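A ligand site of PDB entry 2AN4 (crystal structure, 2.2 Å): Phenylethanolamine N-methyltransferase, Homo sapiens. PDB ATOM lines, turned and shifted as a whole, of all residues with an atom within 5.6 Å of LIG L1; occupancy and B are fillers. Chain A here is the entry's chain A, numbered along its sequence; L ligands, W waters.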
ATOM      1  N   ALA A  24      30.867  16.141   8.551  1.00  0.00           N
ATOM      2  CA  ALA A  24      31.143  17.342   7.699  1.00  0.00           C
ATOM      3  C   ALA A  24      32.162  16.978   6.632  1.00  0.00           C
ATOM      4  O   ALA A  24      31.944  17.226   5.439  1.00  0.00           O
ATOM      5  CB  ALA A  24      31.659  18.491   8.559  1.00  0.00           C
ATOM      6  N   TYR A  27      31.041  13.665   4.722  1.00  0.00           N
ATOM      7  CA  TYR A  27      30.020  13.985   3.732  1.00  0.00           C
ATOM      8  C   TYR A  27      30.550  14.640   2.474  1.00  0.00           C
ATOM      9  O   TYR A  27      29.793  14.880   1.518  1.00  0.00           O
ATOM     10  CB  TYR A  27      28.925  14.865   4.353  1.00  0.00           C
ATOM     11  CG  TYR A  27      27.876  14.062   5.097  1.00  0.00           C
ATOM     12  CD1 TYR A  27      27.969  13.827   6.468  1.00  0.00           C
ATOM     13  CD2 TYR A  27      26.818  13.482   4.401  1.00  0.00           C
ATOM     14  CE1 TYR A  27      27.030  13.042   7.135  1.00  0.00           C
ATOM     15  CE2 TYR A  27      25.873  12.685   5.064  1.00  0.00           C
ATOM     16  CZ  TYR A  27      25.993  12.477   6.414  1.00  0.00           C
ATOM     17  OH  TYR A  27      25.054  11.693   7.051  1.00  0.00           O
ATOM     18  N   PHE A  30      30.142  12.308  -0.383  1.00  0.00           N
ATOM     19  CA  PHE A  30      28.743  11.894  -0.545  1.00  0.00           C
ATOM     20  C   PHE A  30      28.241  12.005  -1.989  1.00  0.00           C
ATOM     21  O   PHE A  30      28.237  13.095  -2.573  1.00  0.00           O
ATOM     22  CB  PHE A  30      27.868  12.771   0.371  1.00  0.00           C
ATOM     23  CG  PHE A  30      26.423  12.361   0.404  1.00  0.00           C
ATOM     24  CD1 PHE A  30      25.959  11.457   1.350  1.00  0.00           C
ATOM     25  CD2 PHE A  30      25.504  12.924  -0.480  1.00  0.00           C
ATOM     26  CE1 PHE A  30      24.618  11.109   1.418  1.00  0.00           C
ATOM     27  CE2 PHE A  30      24.150  12.580  -0.429  1.00  0.00           C
ATOM     28  CZ  PHE A  30      23.707  11.670   0.528  1.00  0.00           C
ATOM     29  N   TYR A  35      23.284   7.532  -3.323  1.00  0.00           N
ATOM     30  CA  TYR A  35      22.381   7.465  -2.189  1.00  0.00           C
ATOM     31  C   TYR A  35      20.983   7.092  -2.690  1.00  0.00           C
ATOM     32  O   TYR A  35      20.360   6.162  -2.180  1.00  0.00           O
ATOM     33  CB  TYR A  35      22.332   8.823  -1.465  1.00  0.00           C
ATOM     34  CG  TYR A  35      21.369   8.832  -0.307  1.00  0.00           C
ATOM     35  CD1 TYR A  35      21.660   8.135   0.873  1.00  0.00           C
ATOM     36  CD2 TYR A  35      20.146   9.498  -0.397  1.00  0.00           C
ATOM     37  CE1 TYR A  35      20.749   8.110   1.942  1.00  0.00           C
ATOM     38  CE2 TYR A  35      19.235   9.479   0.656  1.00  0.00           C
ATOM     39  CZ  TYR A  35      19.539   8.788   1.820  1.00  0.00           C
ATOM     40  OH  TYR A  35      18.675   8.795   2.876  1.00  0.00           O
ATOM     41  N   TYR A  40      16.287   4.384  -2.900  1.00  0.00           N
ATOM     42  CA  TYR A  40      15.046   4.723  -3.559  1.00  0.00           C
ATOM     43  C   TYR A  40      14.834   4.105  -4.933  1.00  0.00           C
ATOM     44  O   TYR A  40      14.015   4.559  -5.723  1.00  0.00           O
ATOM     45  CB  TYR A  40      14.912   6.250  -3.584  1.00  0.00           C
ATOM     46  CG  TYR A  40      14.867   6.783  -2.170  1.00  0.00           C
ATOM     47  CD1 TYR A  40      16.032   7.207  -1.535  1.00  0.00           C
ATOM     48  CD2 TYR A  40      13.681   6.775  -1.435  1.00  0.00           C
ATOM     49  CE1 TYR A  40      16.020   7.599  -0.179  1.00  0.00           C
ATOM     50  CE2 TYR A  40      13.655   7.170  -0.096  1.00  0.00           C
ATOM     51  CZ  TYR A  40      14.815   7.578   0.521  1.00  0.00           C
ATOM     52  OH  TYR A  40      14.772   7.946   1.844  1.00  0.00           O
ATOM     53  N   ASP A  77      11.793  21.695   5.425  1.00  0.00           N
ATOM     54  CA  ASP A  77      12.262  20.311   5.399  1.00  0.00           C
ATOM     55  C   ASP A  77      13.750  20.359   5.710  1.00  0.00           C
ATOM     56  O   ASP A  77      14.522  20.959   4.973  1.00  0.00           O
ATOM     57  CB  ASP A  77      12.009  19.693   4.006  1.00  0.00           C
ATOM     58  CG  ASP A  77      12.448  18.232   3.912  1.00  0.00           C
ATOM     59  OD1 ASP A  77      12.290  17.498   4.908  1.00  0.00           O
ATOM     60  OD2 ASP A  77      12.945  17.819   2.843  1.00  0.00           O
ATOM     61  N   ILE A  78      14.121  19.735   6.831  1.00  0.00           N
ATOM     62  CA  ILE A  78      15.507  19.723   7.314  1.00  0.00           C
ATOM     63  C   ILE A  78      16.349  18.571   6.776  1.00  0.00           C
ATOM     64  O   ILE A  78      16.032  17.404   7.007  1.00  0.00           O
ATOM     65  CB  ILE A  78      15.539  19.638   8.849  1.00  0.00           C
ATOM     66  CG1 ILE A  78      14.636  20.726   9.438  1.00  0.00           C
ATOM     67  CG2 ILE A  78      16.969  19.794   9.352  1.00  0.00           C
ATOM     68  CD1 ILE A  78      14.997  22.116   8.995  1.00  0.00           C
ATOM     69  N   GLY A  79      17.432  18.920   6.084  1.00  0.00           N
ATOM     70  CA  GLY A  79      18.323  17.914   5.527  1.00  0.00           C
ATOM     71  C   GLY A  79      17.612  17.072   4.496  1.00  0.00           C
ATOM     72  O   GLY A  79      17.536  15.841   4.620  1.00  0.00           O
ATOM     73  N   SER A  80      17.088  17.742   3.467  1.00  0.00           N
ATOM     74  CA  SER A  80      16.358  17.099   2.373  1.00  0.00           C
ATOM     75  C   SER A  80      17.228  16.138   1.594  1.00  0.00           C
ATOM     76  O   SER A  80      16.728  15.147   1.035  1.00  0.00           O
ATOM     77  CB  SER A  80      15.809  18.155   1.409  1.00  0.00           C
ATOM     78  OG  SER A  80      14.951  19.066   2.056  1.00  0.00           O
ATOM     79  N   GLY A  81      18.526  16.411   1.537  1.00  0.00           N
ATOM     80  CA  GLY A  81      19.385  15.553   0.755  1.00  0.00           C
ATOM     81  C   GLY A  81      18.861  15.648  -0.664  1.00  0.00           C
ATOM     82  O   GLY A  81      18.350  16.711  -1.048  1.00  0.00           O
ATOM     83  N   PRO A  82      18.959  14.595  -1.469  1.00  0.00           N
ATOM     84  CA  PRO A  82      18.446  14.695  -2.844  1.00  0.00           C
ATOM     85  C   PRO A  82      17.049  14.080  -3.011  1.00  0.00           C
ATOM     86  O   PRO A  82      16.701  13.653  -4.099  1.00  0.00           O
ATOM     87  CB  PRO A  82      19.494  13.935  -3.639  1.00  0.00           C
ATOM     88  CG  PRO A  82      19.801  12.777  -2.725  1.00  0.00           C
ATOM     89  CD  PRO A  82      19.823  13.410  -1.313  1.00  0.00           C
ATOM     90  N   THR A  83      16.262  14.033  -1.947  1.00  0.00           N
ATOM     91  CA  THR A  83      14.949  13.401  -2.057  1.00  0.00           C
ATOM     92  C   THR A  83      13.743  14.312  -1.811  1.00  0.00           C
ATOM     93  O   THR A  83      13.816  15.242  -1.012  1.00  0.00           O
ATOM     94  CB  THR A  83      14.829  12.202  -1.079  1.00  0.00           C
ATOM     95  OG1 THR A  83      14.601  12.692   0.250  1.00  0.00           O
ATOM     96  CG2 THR A  83      16.094  11.355  -1.109  1.00  0.00           C
ATOM     97  N   TYR A  85      10.270  12.659  -1.773  1.00  0.00           N
ATOM     98  CA  TYR A  85       9.173  11.796  -1.311  1.00  0.00           C
ATOM     99  C   TYR A  85       8.566  12.222   0.033  1.00  0.00           C
ATOM    100  O   TYR A  85       7.356  12.110   0.241  1.00  0.00           O
ATOM    101  CB  TYR A  85       9.650  10.338  -1.203  1.00  0.00           C
ATOM    102  CG  TYR A  85      10.418  10.049   0.059  1.00  0.00           C
ATOM    103  CD1 TYR A  85       9.750   9.818   1.271  1.00  0.00           C
ATOM    104  CD2 TYR A  85      11.808  10.101   0.078  1.00  0.00           C
ATOM    105  CE1 TYR A  85      10.444   9.653   2.452  1.00  0.00           C
ATOM    106  CE2 TYR A  85      12.522   9.941   1.266  1.00  0.00           C
ATOM    107  CZ  TYR A  85      11.834   9.712   2.454  1.00  0.00           C
ATOM    108  OH  TYR A  85      12.516   9.532   3.623  1.00  0.00           O
ATOM    109  N   GLN A  86       9.412  12.691   0.937  1.00  0.00           N
ATOM    110  CA  GLN A  86       8.971  13.106   2.263  1.00  0.00           C
ATOM    111  C   GLN A  86       8.031  14.321   2.261  1.00  0.00           C
ATOM    112  O   GLN A  86       7.457  14.666   3.299  1.00  0.00           O
ATOM    113  CB  GLN A  86      10.184  13.424   3.149  1.00  0.00           C
ATOM    114  CG  GLN A  86      10.972  14.676   2.742  1.00  0.00           C
ATOM    115  CD  GLN A  86      12.147  14.371   1.819  1.00  0.00           C
ATOM    116  OE1 GLN A  86      12.178  13.349   1.132  1.00  0.00           O
ATOM    117  NE2 GLN A  86      13.131  15.268   1.797  1.00  0.00           N
ATOM    118  N   ASP A 101      19.652  21.549   2.758  1.00  0.00           N
ATOM    119  CA  ASP A 101      20.708  20.559   2.805  1.00  0.00           C
ATOM    120  C   ASP A 101      22.085  21.166   2.951  1.00  0.00           C
ATOM    121  O   ASP A 101      22.362  22.256   2.451  1.00  0.00           O
ATOM    122  CB  ASP A 101      20.713  19.644   1.593  1.00  0.00           C
ATOM    123  CG  ASP A 101      21.502  18.382   1.862  1.00  0.00           C
ATOM    124  OD1 ASP A 101      21.044  17.595   2.714  1.00  0.00           O
ATOM    125  OD2 ASP A 101      22.577  18.183   1.240  1.00  0.00           O
ATOM    126  N   PHE A 102      22.941  20.435   3.651  1.00  0.00           N
ATOM    127  CA  PHE A 102      24.316  20.816   3.917  1.00  0.00           C
ATOM    128  C   PHE A 102      25.189  20.832   2.662  1.00  0.00           C
ATOM    129  O   PHE A 102      26.086  21.665   2.533  1.00  0.00           O
ATOM    130  CB  PHE A 102      24.905  19.827   4.916  1.00  0.00           C
ATOM    131  CG  PHE A 102      26.257  20.218   5.452  1.00  0.00           C
ATOM    132  CD1 PHE A 102      26.359  21.057   6.556  1.00  0.00           C
ATOM    133  CD2 PHE A 102      27.420  19.733   4.865  1.00  0.00           C
ATOM    134  CE1 PHE A 102      27.611  21.391   7.077  1.00  0.00           C
ATOM    135  CE2 PHE A 102      28.673  20.063   5.373  1.00  0.00           C
ATOM    136  CZ  PHE A 102      28.768  20.903   6.483  1.00  0.00           C
ATOM    137  N   LEU A 103      24.929  19.911   1.747  1.00  0.00           N
ATOM    138  CA  LEU A 103      25.734  19.806   0.530  1.00  0.00           C
ATOM    139  C   LEU A 103      25.193  20.482  -0.710  1.00  0.00           C
ATOM    140  O   LEU A 103      24.025  20.331  -1.073  1.00  0.00           O
ATOM    141  CB  LEU A 103      25.981  18.329   0.208  1.00  0.00           C
ATOM    142  CG  LEU A 103      26.755  17.519   1.251  1.00  0.00           C
ATOM    143  CD1 LEU A 103      26.829  16.058   0.798  1.00  0.00           C
ATOM    144  CD2 LEU A 103      28.146  18.111   1.447  1.00  0.00           C
ATOM    145  N   ASN A 106      23.765  18.160  -3.328  1.00  0.00           N
ATOM    146  CA  ASN A 106      22.400  17.704  -3.096  1.00  0.00           C
ATOM    147  C   ASN A 106      21.412  18.744  -3.575  1.00  0.00           C
ATOM    148  O   ASN A 106      20.476  18.433  -4.320  1.00  0.00           O
ATOM    149  CB  ASN A 106      22.166  17.408  -1.617  1.00  0.00           C
ATOM    150  CG  ASN A 106      22.693  16.052  -1.201  1.00  0.00           C
ATOM    151  OD1 ASN A 106      22.578  15.091  -1.950  1.00  0.00           O
ATOM    152  ND2 ASN A 106      23.242  15.967   0.009  1.00  0.00           N
ATOM    153  N   ILE A 157      22.162  24.483   5.056  1.00  0.00           N
ATOM    154  CA  ILE A 157      21.773  24.345   6.443  1.00  0.00           C
ATOM    155  C   ILE A 157      22.774  23.497   7.199  1.00  0.00           C
ATOM    156  O   ILE A 157      23.449  22.644   6.621  1.00  0.00           O
ATOM    157  CB  ILE A 157      20.349  23.712   6.531  1.00  0.00           C
ATOM    158  CG1 ILE A 157      19.859  23.687   7.979  1.00  0.00           C
ATOM    159  CG2 ILE A 157      20.384  22.284   5.960  1.00  0.00           C
ATOM    160  CD1 ILE A 157      18.443  23.140   8.138  1.00  0.00           C
ATOM    161  N   ASP A 158      22.879  23.757   8.501  1.00  0.00           N
ATOM    162  CA  ASP A 158      23.777  23.008   9.366  1.00  0.00           C
ATOM    163  C   ASP A 158      23.077  22.868  10.711  1.00  0.00           C
ATOM    164  O   ASP A 158      23.020  23.823  11.491  1.00  0.00           O
ATOM    165  CB  ASP A 158      25.087  23.760   9.558  1.00  0.00           C
ATOM    166  CG  ASP A 158      26.156  22.912  10.223  1.00  0.00           C
ATOM    167  OD1 ASP A 158      25.828  22.183  11.188  1.00  0.00           O
ATOM    168  OD2 ASP A 158      27.327  22.980   9.788  1.00  0.00           O
ATOM    169  N   VAL A 159      22.539  21.681  10.980  1.00  0.00           N
ATOM    170  CA  VAL A 159      21.816  21.479  12.231  1.00  0.00           C
ATOM    171  C   VAL A 159      22.695  21.611  13.464  1.00  0.00           C
ATOM    172  O   VAL A 159      22.188  21.649  14.579  1.00  0.00           O
ATOM    173  CB  VAL A 159      21.122  20.091  12.243  1.00  0.00           C
ATOM    174  CG1 VAL A 159      20.056  20.037  11.148  1.00  0.00           C
ATOM    175  CG2 VAL A 159      22.154  18.986  12.064  1.00  0.00           C
ATOM    176  N   HIS A 160      24.000  21.703  13.263  1.00  0.00           N
ATOM    177  CA  HIS A 160      24.914  21.828  14.397  1.00  0.00           C
ATOM    178  C   HIS A 160      25.047  23.266  14.883  1.00  0.00           C
ATOM    179  O   HIS A 160      25.572  23.518  15.966  1.00  0.00           O
ATOM    180  CB  HIS A 160      26.267  21.245  14.042  1.00  0.00           C
ATOM    181  CG  HIS A 160      26.232  19.785  13.757  1.00  0.00           C
ATOM    182  ND1 HIS A 160      25.616  18.886  14.599  1.00  0.00           N
ATOM    183  CD2 HIS A 160      26.712  19.062  12.714  1.00  0.00           C
ATOM    184  CE1 HIS A 160      25.715  17.674  14.094  1.00  0.00           C
ATOM    185  NE2 HIS A 160      26.376  17.747  12.951  1.00  0.00           N
ATOM    186  N   ALA A 181      13.838  13.792   7.458  1.00  0.00           N
ATOM    187  CA  ALA A 181      13.980  12.353   7.286  1.00  0.00           C
ATOM    188  C   ALA A 181      15.435  11.907   7.137  1.00  0.00           C
ATOM    189  O   ALA A 181      16.134  12.343   6.235  1.00  0.00           O
ATOM    190  CB  ALA A 181      13.158  11.892   6.063  1.00  0.00           C
ATOM    191  N   PHE A 182      15.866  11.043   8.046  1.00  0.00           N
ATOM    192  CA  PHE A 182      17.230  10.508   8.042  1.00  0.00           C
ATOM    193  C   PHE A 182      18.330  11.561   8.049  1.00  0.00           C
ATOM    194  O   PHE A 182      19.323  11.444   7.343  1.00  0.00           O
ATOM    195  CB  PHE A 182      17.415   9.577   6.829  1.00  0.00           C
ATOM    196  CG  PHE A 182      16.392   8.507   6.744  1.00  0.00           C
ATOM    197  CD1 PHE A 182      15.263   8.675   5.940  1.00  0.00           C
ATOM    198  CD2 PHE A 182      16.508   7.348   7.508  1.00  0.00           C
ATOM    199  CE1 PHE A 182      14.277   7.696   5.898  1.00  0.00           C
ATOM    200  CE2 PHE A 182      15.522   6.368   7.466  1.00  0.00           C
ATOM    201  CZ  PHE A 182      14.406   6.547   6.660  1.00  0.00           C
ATOM    202  N   CYS A 183      18.148  12.604   8.850  1.00  0.00           N
ATOM    203  CA  CYS A 183      19.178  13.624   8.906  1.00  0.00           C
ATOM    204  C   CYS A 183      19.910  13.626  10.239  1.00  0.00           C
ATOM    205  O   CYS A 183      21.079  13.265  10.313  1.00  0.00           O
ATOM    206  CB  CYS A 183      18.589  15.012   8.646  1.00  0.00           C
ATOM    207  SG  CYS A 183      19.850  16.321   8.716  1.00  0.00           S
ATOM    208  N   ALA A 186      21.991  10.830  11.232  1.00  0.00           N
ATOM    209  CA  ALA A 186      23.034  10.604  10.229  1.00  0.00           C
ATOM    210  C   ALA A 186      24.118  11.669  10.247  1.00  0.00           C
ATOM    211  O   ALA A 186      25.096  11.565   9.520  1.00  0.00           O
ATOM    212  CB  ALA A 186      22.399  10.529   8.838  1.00  0.00           C
ATOM    213  N   VAL A 187      23.958  12.687  11.094  1.00  0.00           N
ATOM    214  CA  VAL A 187      24.938  13.762  11.173  1.00  0.00           C
ATOM    215  C   VAL A 187      25.490  13.990  12.577  1.00  0.00           C
ATOM    216  O   VAL A 187      26.242  14.932  12.803  1.00  0.00           O
ATOM    217  CB  VAL A 187      24.327  15.081  10.665  1.00  0.00           C
ATOM    218  CG1 VAL A 187      23.764  14.882   9.258  1.00  0.00           C
ATOM    219  CG2 VAL A 187      23.232  15.550  11.619  1.00  0.00           C
ATOM    220  N   TYR A 222      26.058   3.789   6.670  1.00  0.00           N
ATOM    221  CA  TYR A 222      25.340   3.623   5.417  1.00  0.00           C
ATOM    222  C   TYR A 222      26.257   4.232   4.364  1.00  0.00           C
ATOM    223  O   TYR A 222      27.004   5.190   4.643  1.00  0.00           O
ATOM    224  CB  TYR A 222      23.959   4.303   5.451  1.00  0.00           C
ATOM    225  CG  TYR A 222      23.942   5.807   5.288  1.00  0.00           C
ATOM    226  CD1 TYR A 222      23.954   6.390   4.020  1.00  0.00           C
ATOM    227  CD2 TYR A 222      23.937   6.641   6.406  1.00  0.00           C
ATOM    228  CE1 TYR A 222      23.965   7.774   3.867  1.00  0.00           C
ATOM    229  CE2 TYR A 222      23.946   8.038   6.263  1.00  0.00           C
ATOM    230  CZ  TYR A 222      23.954   8.590   4.997  1.00  0.00           C
ATOM    231  OH  TYR A 222      23.974   9.953   4.843  1.00  0.00           O
HETATM  232  N1  LIG L   1      16.171  13.404   3.801  1.00  0.00           N
HETATM  233  C1  LIG L   1      16.596  12.483   2.747  1.00  0.00           C
HETATM  234  C2  LIG L   1      18.157  12.444   2.690  1.00  0.00           C
HETATM  235  C3  LIG L   1      18.887  12.140   4.020  1.00  0.00           C
HETATM  236  S1  LIG L   1      20.689  11.881   3.792  1.00  0.00           S
HETATM  237  C4  LIG L   1      15.989  11.084   2.896  1.00  0.00           C
HETATM  238  O1  LIG L   1      16.575  10.093   2.412  1.00  0.00           O
HETATM  239  O2  LIG L   1      14.878  10.981   3.474  1.00  0.00           O
HETATM  240  C5  LIG L   1      21.405  12.933   5.087  1.00  0.00           C
HETATM  241  C6  LIG L   1      21.641  14.330   4.571  1.00  0.00           C
HETATM  242  O3  LIG L   1      22.087  15.236   5.618  1.00  0.00           O
HETATM  243  C7  LIG L   1      22.613  14.489   3.407  1.00  0.00           C
HETATM  244  O4  LIG L   1      21.965  15.102   2.302  1.00  0.00           O
HETATM  245  C8  LIG L   1      23.748  15.329   4.002  1.00  0.00           C
HETATM  246  O5  LIG L   1      24.418  16.166   3.080  1.00  0.00           O
HETATM  247  C9  LIG L   1      23.007  16.147   5.059  1.00  0.00           C
HETATM  248  N2  LIG L   1      23.855  16.707   6.121  1.00  0.00           N
HETATM  249  C10 LIG L   1      25.218  16.401   6.447  1.00  0.00           C
HETATM  250  N3  LIG L   1      25.693  17.150   7.419  1.00  0.00           N
HETATM  251  C11 LIG L   1      24.609  17.947   7.770  1.00  0.00           C
HETATM  252  C12 LIG L   1      24.541  18.961   8.745  1.00  0.00           C
HETATM  253  N4  LIG L   1      25.555  19.323   9.527  1.00  0.00           N
HETATM  254  N5  LIG L   1      23.349  19.618   8.884  1.00  0.00           N
HETATM  255  C13 LIG L   1      22.315  19.258   8.078  1.00  0.00           C
HETATM  256  N6  LIG L   1      22.282  18.310   7.110  1.00  0.00           N
HETATM  257  C14 LIG L   1      23.483  17.686   7.007  1.00  0.00           C
HETATM  258  C1  LG2 L   2      17.682   3.435   5.511  1.00  0.00           C
HETATM  259  C2  LG2 L   2      16.582   2.878   4.870  1.00  0.00           C
HETATM  260  C3  LG2 L   2      15.891   3.607   3.912  1.00  0.00           C
HETATM  261  O1  LG2 L   2      14.818   3.057   3.286  1.00  0.00           O
HETATM  262  C4  LG2 L   2      16.297   4.906   3.604  1.00  0.00           C
HETATM  263  C5  LG2 L   2      17.404   5.456   4.255  1.00  0.00           C
HETATM  264  C6  LG2 L   2      18.095   4.727   5.214  1.00  0.00           C
HETATM  265  C7  LG2 L   2      19.302   5.302   5.947  1.00  0.00           C
HETATM  266  O2  LG2 L   2      20.497   4.653   5.495  1.00  0.00           O
HETATM  267  C8  LG2 L   2      19.437   6.814   5.729  1.00  0.00           C
HETATM  268  N1  LG2 L   2      20.623   7.321   6.452  1.00  0.00           N
HETATM  269  O   HOH W   1      14.320  15.611   5.122  1.00  0.00           O
HETATM  270  O   HOH W   2      28.743  18.813  10.634  1.00  0.00           O
HETATM  271  O   HOH W   3      28.271  17.385   8.401  1.00  0.00           O
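Tyr 27 touches LIG L1.
Gly 81 touches LIG L1 (CA to O4, 3.0 Å).
Thr 83 touches LIG L1 (OG1 to C1, 3.2 Å).
Phe 102 touches LIG L1.
CG of Leu 103 touches O5 of LIG L1 (3.3 Å).
Ile 157 touches LIG L1.
CD2 of His 160 touches N4 of LIG L1, at 3.4 Å.
Phe 182 touches LIG L1 (CD1 to O2, 3.4 Å).
Val 187 touches LIG L1 (CG1 to N3, 3.5 Å).
Tyr 222 touches LIG L1 (OH to C5, 3.9 Å).
Of the 28 residues printed, 21 come within 4 Å of LIG L1.
Along chain A the residues within 4 Å of LIG L1 span positions 27 to 222.
Water W3 bridges N3 of LIG L1 (2.8 Å) and N of Ala 24 (2.9 Å).
Water W2 lies within hydrogen-bond range of N4 of LIG L1 (3.4 Å) and NE2 of His 160 (3.5 Å).
OH of Tyr 35 sits at hydrogen-bond distance from O1 of LIG L1, at 2.5 Å.
An oxygen (O4) of LIG L1 lies within hydrogen-bond range of the side-chain amide nitrogen (ND2) of Asn 106, at 2.8 Å.
OD1 of Asp 101 is in hydrogen-bond range of O4 of LIG L1, 2.7 Å away.
The backbone carbonyl oxygen (O) of Gly 79 is in hydrogen-bond range of a nitrogen (N1) of LIG L1, 2.9 Å away.
The backbone carbonyl oxygen (O) of Ala 181 is in hydrogen-bond range of a nitrogen (N1) of LIG L1, at 2.7 Å.
The side-chain sulfur (SG) of Cys 183 lies within hydrogen-bond range of a nitrogen (N6) of LIG L1 (3.5 Å).
An oxygen (O2) of LIG L1 sits at hydrogen-bond distance from the side-chain hydroxyl of Tyr 85 (2.8 Å).
The backbone carbonyl oxygen (O) of Ser 80 sits close to a nitrogen (N1) of LIG L1.
OD1 of Asp 158 is in hydrogen-bond range of N4 of LIG L1.
An oxygen (O1) of LIG L1 is in hydrogen-bond range of the side-chain hydroxyl of Tyr 40 (2.9 Å).
The backbone NH of Val 159 lies within hydrogen-bond range of a nitrogen (N5) of LIG L1, 3.1 Å away.
The backbone NH (N) of Ile 157 sits at hydrogen-bond distance from the backbone carbonyl oxygen (O) of Asp 101 (3.4 Å).
The side-chain amide oxygen (OE1) of Gln 86 is in hydrogen-bond range of the side-chain hydroxyl (OG1) of Thr 83, at 2.7 Å.
The backbone NH of Gly 81 is in hydrogen-bond range of the side-chain carboxylate of Asp 101 (3.0 Å).
OH of Tyr 222 lies within hydrogen-bond range of OH of Tyr 27.
OG1 of Thr 83 sits at hydrogen-bond distance from O of Ser 80, at 3.3 Å.
The backbone NH of His 160 sits at hydrogen-bond distance from the side-chain carboxylate of Asp 158 (2.8 Å).
The side-chain hydroxyl (OH) of Tyr 85 sits close to the side-chain hydroxyl (OH) of Tyr 40, 3.3 Å away.
OD2 of Asp 101 is in hydrogen-bond range of N of Leu 103, 3.0 Å away.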
